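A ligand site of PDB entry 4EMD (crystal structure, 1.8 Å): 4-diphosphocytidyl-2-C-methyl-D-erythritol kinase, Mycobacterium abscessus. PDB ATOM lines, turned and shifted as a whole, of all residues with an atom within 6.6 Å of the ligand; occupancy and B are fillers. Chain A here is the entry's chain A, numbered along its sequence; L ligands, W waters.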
ATOM      1  N   VAL A  32      26.673 -28.186   5.733  1.00  0.00           N
ATOM      2  CA  VAL A  32      26.117 -26.958   6.320  1.00  0.00           C
ATOM      3  C   VAL A  32      24.853 -27.328   7.073  1.00  0.00           C
ATOM      4  O   VAL A  32      23.937 -27.930   6.490  1.00  0.00           O
ATOM      5  CB  VAL A  32      25.848 -25.886   5.256  1.00  0.00           C
ATOM      6  CG1 VAL A  32      25.180 -24.632   5.918  1.00  0.00           C
ATOM      7  CG2 VAL A  32      27.146 -25.522   4.544  1.00  0.00           C
ATOM      8  N   LEU A  35      20.972 -22.649  10.927  1.00  0.00           N
ATOM      9  CA  LEU A  35      21.267 -21.277  11.369  1.00  0.00           C
ATOM     10  C   LEU A  35      21.177 -21.183  12.914  1.00  0.00           C
ATOM     11  O   LEU A  35      20.159 -21.551  13.490  1.00  0.00           O
ATOM     12  CB  LEU A  35      20.299 -20.287  10.677  1.00  0.00           C
ATOM     13  CG  LEU A  35      20.603 -18.770  10.724  1.00  0.00           C
ATOM     14  CD1 LEU A  35      22.013 -18.433  10.257  1.00  0.00           C
ATOM     15  CD2 LEU A  35      19.581 -18.044   9.868  1.00  0.00           C
ATOM     16  N   ARG A  36      22.253 -20.737  13.548  1.00  0.00           N
ATOM     17  CA  ARG A  36      22.372 -20.646  15.011  1.00  0.00           C
ATOM     18  C   ARG A  36      21.853 -19.302  15.537  1.00  0.00           C
ATOM     19  O   ARG A  36      21.681 -18.344  14.748  1.00  0.00           O
ATOM     20  CB  ARG A  36      23.851 -20.756  15.443  1.00  0.00           C
ATOM     21  CG  ARG A  36      24.455 -22.155  15.373  1.00  0.00           C
ATOM     22  CD  ARG A  36      25.930 -22.128  14.940  1.00  0.00           C
ATOM     23  NE  ARG A  36      26.815 -21.266  15.740  1.00  0.00           N
ATOM     24  CZ  ARG A  36      27.914 -21.684  16.391  1.00  0.00           C
ATOM     25  NH1 ARG A  36      28.304 -22.951  16.367  1.00  0.00           N
ATOM     26  NH2 ARG A  36      28.642 -20.801  17.076  1.00  0.00           N
ATOM     27  N   GLY A  39      23.767 -16.112  14.451  1.00  0.00           N
ATOM     28  CA  GLY A  39      23.693 -15.688  13.027  1.00  0.00           C
ATOM     29  C   GLY A  39      24.624 -16.465  12.073  1.00  0.00           C
ATOM     30  O   GLY A  39      24.651 -16.219  10.848  1.00  0.00           O
ATOM     31  N   TYR A  40      25.405 -17.384  12.639  1.00  0.00           N
ATOM     32  CA  TYR A  40      26.223 -18.330  11.850  1.00  0.00           C
ATOM     33  C   TYR A  40      25.491 -19.659  11.667  1.00  0.00           C
ATOM     34  O   TYR A  40      24.578 -20.012  12.421  1.00  0.00           O
ATOM     35  CB  TYR A  40      27.557 -18.606  12.546  1.00  0.00           C
ATOM     36  CG  TYR A  40      28.433 -17.398  12.508  1.00  0.00           C
ATOM     37  CD1 TYR A  40      29.316 -17.182  11.479  1.00  0.00           C
ATOM     38  CD2 TYR A  40      28.319 -16.418  13.501  1.00  0.00           C
ATOM     39  CE1 TYR A  40      30.093 -16.038  11.433  1.00  0.00           C
ATOM     40  CE2 TYR A  40      29.079 -15.267  13.461  1.00  0.00           C
ATOM     41  CZ  TYR A  40      29.956 -15.077  12.416  1.00  0.00           C
ATOM     42  OH  TYR A  40      30.716 -13.926  12.376  1.00  0.00           O
ATOM     43  N   HIS A  41      25.909 -20.402  10.641  1.00  0.00           N
ATOM     44  CA  HIS A  41      25.458 -21.757  10.474  1.00  0.00           C
ATOM     45  C   HIS A  41      26.389 -22.728  11.171  1.00  0.00           C
ATOM     46  O   HIS A  41      27.649 -22.588  11.116  1.00  0.00           O
ATOM     47  CB  HIS A  41      25.413 -22.116   8.988  1.00  0.00           C
ATOM     48  CG  HIS A  41      24.349 -21.355   8.230  1.00  0.00           C
ATOM     49  ND1 HIS A  41      24.464 -20.043   7.925  1.00  0.00           N
ATOM     50  CD2 HIS A  41      23.133 -21.783   7.692  1.00  0.00           C
ATOM     51  CE1 HIS A  41      23.360 -19.651   7.257  1.00  0.00           C
ATOM     52  NE2 HIS A  41      22.547 -20.694   7.122  1.00  0.00           N
ATOM     53  N   GLU A  42      25.815 -23.754  11.772  1.00  0.00           N
ATOM     54  CA  GLU A  42      26.588 -24.853  12.271  1.00  0.00           C
ATOM     55  C   GLU A  42      27.155 -25.569  11.058  1.00  0.00           C
ATOM     56  O   GLU A  42      26.507 -25.653  10.019  1.00  0.00           O
ATOM     57  CB  GLU A  42      25.744 -25.796  13.106  1.00  0.00           C
ATOM     58  CG  GLU A  42      26.583 -26.853  13.804  1.00  0.00           C
ATOM     59  CD  GLU A  42      27.341 -26.348  15.041  1.00  0.00           C
ATOM     60  OE1 GLU A  42      27.076 -25.208  15.556  1.00  0.00           O
ATOM     61  OE2 GLU A  42      28.226 -27.110  15.495  1.00  0.00           O
ATOM     62  N   LEU A  43      28.403 -26.010  11.134  1.00  0.00           N
ATOM     63  CA  LEU A  43      28.929 -26.763  10.009  1.00  0.00           C
ATOM     64  C   LEU A  43      29.963 -27.814  10.417  1.00  0.00           C
ATOM     65  O   LEU A  43      30.457 -27.808  11.529  1.00  0.00           O
ATOM     66  CB  LEU A  43      29.478 -25.827   8.935  1.00  0.00           C
ATOM     67  CG  LEU A  43      30.524 -24.825   9.320  1.00  0.00           C
ATOM     68  CD1 LEU A  43      31.784 -25.604   9.536  1.00  0.00           C
ATOM     69  CD2 LEU A  43      30.762 -23.744   8.262  1.00  0.00           C
ATOM     70  N   LEU A  83      40.130  -7.124   6.657  1.00  0.00           N
ATOM     71  CA  LEU A  83      40.196  -7.934   7.871  1.00  0.00           C
ATOM     72  C   LEU A  83      41.604  -7.813   8.504  1.00  0.00           C
ATOM     73  O   LEU A  83      41.777  -8.003   9.712  1.00  0.00           O
ATOM     74  CB  LEU A  83      39.824  -9.403   7.612  1.00  0.00           C
ATOM     75  CG  LEU A  83      39.651 -10.306   8.837  1.00  0.00           C
ATOM     76  CD1 LEU A  83      38.543  -9.745   9.741  1.00  0.00           C
ATOM     77  CD2 LEU A  83      39.346 -11.742   8.379  1.00  0.00           C
ATOM     78  N   SER A 119      41.146 -13.961   5.352  1.00  0.00           N
ATOM     79  CA  SER A 119      41.448 -14.710   6.547  1.00  0.00           C
ATOM     80  C   SER A 119      42.899 -15.091   6.642  1.00  0.00           C
ATOM     81  O   SER A 119      43.484 -15.054   7.716  1.00  0.00           O
ATOM     82  CB  SER A 119      40.583 -15.949   6.648  1.00  0.00           C
ATOM     83  OG  SER A 119      39.224 -15.556   6.730  1.00  0.00           O
ATOM     84  N   LEU A 149      38.136 -12.864  14.775  1.00  0.00           N
ATOM     85  CA  LEU A 149      38.218 -12.183  13.488  1.00  0.00           C
ATOM     86  C   LEU A 149      37.329 -12.777  12.432  1.00  0.00           C
ATOM     87  O   LEU A 149      36.731 -12.033  11.655  1.00  0.00           O
ATOM     88  CB  LEU A 149      39.668 -12.160  13.020  1.00  0.00           C
ATOM     89  CG  LEU A 149      40.539 -11.254  13.919  1.00  0.00           C
ATOM     90  CD1 LEU A 149      42.017 -11.540  13.727  1.00  0.00           C
ATOM     91  CD2 LEU A 149      40.246  -9.762  13.697  1.00  0.00           C
ATOM     92  N   GLY A 150      37.203 -14.097  12.399  1.00  0.00           N
ATOM     93  CA  GLY A 150      36.391 -14.744  11.397  1.00  0.00           C
ATOM     94  C   GLY A 150      36.466 -16.254  11.474  1.00  0.00           C
ATOM     95  O   GLY A 150      37.454 -16.797  11.962  1.00  0.00           O
ATOM     96  N   SER A 151      35.470 -16.914  10.898  1.00  0.00           N
ATOM     97  CA  SER A 151      35.325 -18.369  10.936  1.00  0.00           C
ATOM     98  C   SER A 151      36.460 -19.121  10.264  1.00  0.00           C
ATOM     99  O   SER A 151      36.782 -20.246  10.682  1.00  0.00           O
ATOM    100  CB  SER A 151      34.023 -18.791  10.278  1.00  0.00           C
ATOM    101  OG  SER A 151      32.972 -18.177  10.961  1.00  0.00           O
ATOM    102  N   ASP A 152      37.074 -18.525   9.254  1.00  0.00           N
ATOM    103  CA  ASP A 152      38.182 -19.202   8.549  1.00  0.00           C
ATOM    104  C   ASP A 152      39.564 -18.771   9.038  1.00  0.00           C
ATOM    105  O   ASP A 152      40.570 -19.327   8.576  1.00  0.00           O
ATOM    106  CB  ASP A 152      38.133 -18.951   7.012  1.00  0.00           C
ATOM    107  CG  ASP A 152      36.951 -19.609   6.360  1.00  0.00           C
ATOM    108  OD1 ASP A 152      36.525 -20.710   6.793  1.00  0.00           O
ATOM    109  OD2 ASP A 152      36.387 -19.008   5.429  1.00  0.00           O
ATOM    110  N   GLY A 166      31.677 -26.534  14.843  1.00  0.00           N
ATOM    111  CA  GLY A 166      31.071 -25.273  15.289  1.00  0.00           C
ATOM    112  C   GLY A 166      30.674 -24.425  14.095  1.00  0.00           C
ATOM    113  O   GLY A 166      29.875 -24.897  13.275  1.00  0.00           O
ATOM    114  N   ARG A 167      31.179 -23.205  14.028  1.00  0.00           N
ATOM    115  CA  ARG A 167      31.055 -22.357  12.832  1.00  0.00           C
ATOM    116  C   ARG A 167      32.197 -22.586  11.862  1.00  0.00           C
ATOM    117  O   ARG A 167      32.270 -21.888  10.849  1.00  0.00           O
ATOM    118  CB  ARG A 167      31.148 -20.858  13.136  1.00  0.00           C
ATOM    119  CG  ARG A 167      30.585 -20.266  14.377  1.00  0.00           C
ATOM    120  CD  ARG A 167      30.948 -18.780  14.433  1.00  0.00           C
ATOM    121  NE  ARG A 167      32.187 -18.492  15.166  1.00  0.00           N
ATOM    122  CZ  ARG A 167      33.204 -17.719  14.753  1.00  0.00           C
ATOM    123  NH1 ARG A 167      33.205 -17.099  13.566  1.00  0.00           N
ATOM    124  NH2 ARG A 167      34.240 -17.522  15.565  1.00  0.00           N
ATOM    125  N   GLY A 168      33.120 -23.493  12.208  1.00  0.00           N
ATOM    126  CA  GLY A 168      34.364 -23.731  11.438  1.00  0.00           C
ATOM    127  C   GLY A 168      35.641 -23.364  12.217  1.00  0.00           C
ATOM    128  O   GLY A 168      36.776 -23.625  11.740  1.00  0.00           O
ATOM    129  N   THR A 193      30.241 -14.224   0.652  1.00  0.00           N
ATOM    130  CA  THR A 193      29.976 -15.401   1.497  1.00  0.00           C
ATOM    131  C   THR A 193      28.597 -15.352   2.172  1.00  0.00           C
ATOM    132  O   THR A 193      27.874 -16.333   2.150  1.00  0.00           O
ATOM    133  CB  THR A 193      31.088 -15.586   2.547  1.00  0.00           C
ATOM    134  OG1 THR A 193      32.341 -15.727   1.850  1.00  0.00           O
ATOM    135  CG2 THR A 193      30.850 -16.798   3.379  1.00  0.00           C
ATOM    136  N   PRO A 194      28.198 -14.210   2.760  1.00  0.00           N
ATOM    137  CA  PRO A 194      26.837 -14.257   3.311  1.00  0.00           C
ATOM    138  C   PRO A 194      25.695 -14.513   2.305  1.00  0.00           C
ATOM    139  O   PRO A 194      24.672 -15.103   2.680  1.00  0.00           O
ATOM    140  CB  PRO A 194      26.649 -12.900   3.981  1.00  0.00           C
ATOM    141  CG  PRO A 194      27.706 -12.044   3.427  1.00  0.00           C
ATOM    142  CD  PRO A 194      28.830 -12.892   2.933  1.00  0.00           C
ATOM    143  N   GLN A 195      25.847 -14.056   1.058  1.00  0.00           N
ATOM    144  CA  GLN A 195      24.817 -14.334   0.039  1.00  0.00           C
ATOM    145  C   GLN A 195      24.728 -15.820  -0.270  1.00  0.00           C
ATOM    146  O   GLN A 195      23.659 -16.345  -0.479  1.00  0.00           O
ATOM    147  CB  GLN A 195      25.084 -13.547  -1.269  1.00  0.00           C
ATOM    148  CG  GLN A 195      23.953 -13.709  -2.289  1.00  0.00           C
ATOM    149  CD  GLN A 195      24.218 -13.181  -3.714  1.00  0.00           C
ATOM    150  OE1 GLN A 195      25.362 -12.999  -4.171  1.00  0.00           O
ATOM    151  NE2 GLN A 195      23.117 -12.935  -4.428  1.00  0.00           N
ATOM    152  N   PHE A 197      25.511 -18.367   1.768  1.00  0.00           N
ATOM    153  CA  PHE A 197      24.818 -19.034   2.895  1.00  0.00           C
ATOM    154  C   PHE A 197      23.333 -18.702   2.856  1.00  0.00           C
ATOM    155  O   PHE A 197      22.516 -19.581   3.122  1.00  0.00           O
ATOM    156  CB  PHE A 197      25.422 -18.646   4.252  1.00  0.00           C
ATOM    157  CG  PHE A 197      26.629 -19.445   4.627  1.00  0.00           C
ATOM    158  CD1 PHE A 197      26.490 -20.708   5.190  1.00  0.00           C
ATOM    159  CD2 PHE A 197      27.905 -18.935   4.414  1.00  0.00           C
ATOM    160  CE1 PHE A 197      27.603 -21.419   5.583  1.00  0.00           C
ATOM    161  CE2 PHE A 197      29.048 -19.668   4.789  1.00  0.00           C
ATOM    162  CZ  PHE A 197      28.883 -20.902   5.375  1.00  0.00           C
ATOM    163  N   LYS A 198      22.952 -17.495   2.496  1.00  0.00           N
ATOM    164  CA  LYS A 198      21.507 -17.184   2.403  1.00  0.00           C
ATOM    165  C   LYS A 198      20.880 -18.053   1.314  1.00  0.00           C
ATOM    166  O   LYS A 198      19.769 -18.553   1.469  1.00  0.00           O
ATOM    167  CB  LYS A 198      21.243 -15.717   2.103  1.00  0.00           C
HETATM  168  O1  LIG L   1      33.126 -15.725   9.892  1.00  0.00           O
HETATM  169  P1  LIG L   1      32.956 -14.818   8.690  1.00  0.00           P
HETATM  170  O2  LIG L   1      32.923 -13.343   8.991  1.00  0.00           O
HETATM  171  O3  LIG L   1      33.986 -15.037   7.619  1.00  0.00           O
HETATM  172  O4  LIG L   1      31.487 -15.107   8.050  1.00  0.00           O
HETATM  173  C1  LIG L   1      30.944 -14.250   7.042  1.00  0.00           C
HETATM  174  C2  LIG L   1      29.491 -14.536   6.855  1.00  0.00           C
HETATM  175  O5  LIG L   1      29.249 -15.850   6.302  1.00  0.00           O
HETATM  176  C3  LIG L   1      28.707 -14.494   8.147  1.00  0.00           C
HETATM  177  O6  LIG L   1      28.288 -13.188   8.520  1.00  0.00           O
HETATM  178  C4  LIG L   1      27.541 -15.383   7.833  1.00  0.00           C
HETATM  179  O7  LIG L   1      26.608 -14.644   7.084  1.00  0.00           O
HETATM  180  C5  LIG L   1      28.135 -16.436   6.926  1.00  0.00           C
HETATM  181  N1  LIG L   1      28.617 -17.607   7.681  1.00  0.00           N
HETATM  182  C6  LIG L   1      27.706 -18.509   8.156  1.00  0.00           C
HETATM  183  N2  LIG L   1      28.092 -19.613   8.854  1.00  0.00           N
HETATM  184  C7  LIG L   1      29.377 -19.855   9.090  1.00  0.00           C
HETATM  185  C8  LIG L   1      30.363 -18.974   8.594  1.00  0.00           C
HETATM  186  C9  LIG L   1      29.956 -17.841   7.868  1.00  0.00           C
HETATM  187  O8  LIG L   1      26.502 -18.283   7.974  1.00  0.00           O
HETATM  188  N3  LIG L   1      29.715 -20.973   9.796  1.00  0.00           N
HETATM  189  O   HOH W   1      27.883 -11.069   7.042  1.00  0.00           O
HETATM  190  O   HOH W   2      34.172 -13.057   5.473  1.00  0.00           O
HETATM  191  O   HOH W   3      30.676 -12.212   9.843  1.00  0.00           O
HETATM  192  O   HOH W   4      35.304 -11.924   9.373  1.00  0.00           O
HETATM  193  O   HOH W   5      23.961 -15.136   5.273  1.00  0.00           O
HETATM  194  O   HOH W   6      27.036 -13.830  11.455  1.00  0.00           O
HETATM  195  O   HOH W   7      30.478 -10.991   5.858  1.00  0.00           O
HETATM  196  O   HOH W   8      36.943 -15.824   8.312  1.00  0.00           O
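O of Arg 167 is in hydrogen-bond range of N3 of the ligand (2.9 Å).
The backbone carbonyl oxygen (O) of His 41 is in hydrogen-bond range of a nitrogen (N3) of the ligand (2.9 Å).
The guanidinium group of Arg 167 is in salt-bridge range of an oxygen (O1) of the ligand (3.9 Å).
The backbone NH of His 41 lies within hydrogen-bond range of a nitrogen (N2) of the ligand, 2.9 Å away.
OG of Ser 151 lies within hydrogen-bond range of O1 of the ligand (2.7 Å).
N of Ser 151 lies within hydrogen-bond range of O1 of the ligand, at 2.8 Å.
A ring nitrogen (ND1) of His 41 sits at hydrogen-bond distance from an oxygen (O8) of the ligand, at 2.7 Å.
The guanidinium group (NH1) of Arg 167 is in hydrogen-bond range of the side-chain hydroxyl (OG) of Ser 151.
N of Leu 43 is in hydrogen-bond range of O of Gly 166 (2.8 Å).
Merely in contact with the ligand: Leu 43 (3.3 Å), Tyr 40 (3.4 Å), Thr 193 (3.5 Å), Phe 197 (3.5 Å), Pro 194 (3.6 Å), Gly 150 (3.7 Å) and Gly 39 (3.99 Å).
Within 4 Å of the ligand: Gly 39, Tyr 40, His 41, Leu 43, Gly 150, Ser 151, Arg 167, Thr 193, Pro 194 and Phe 197.
Water W3 lies within hydrogen-bond range of O2 of the ligand and OH of Tyr 40.
Water W4 lies within hydrogen-bond range of O of Leu 149 and O2 of the ligand.
Water W8 lies within hydrogen-bond range of OG of Ser 119 (2.8 Å), N of Asp 152 (2.9 Å), O3 of the ligand (3.1 Å) and N of Ser 151 (3.2 Å).
Water W5 bridges the backbone carbonyl oxygen (O) of Pro 194 (2.7 Å) and an oxygen (O7) of the ligand (3.2 Å).
Water W6 bridges O6 of the ligand and O of Gly 39.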
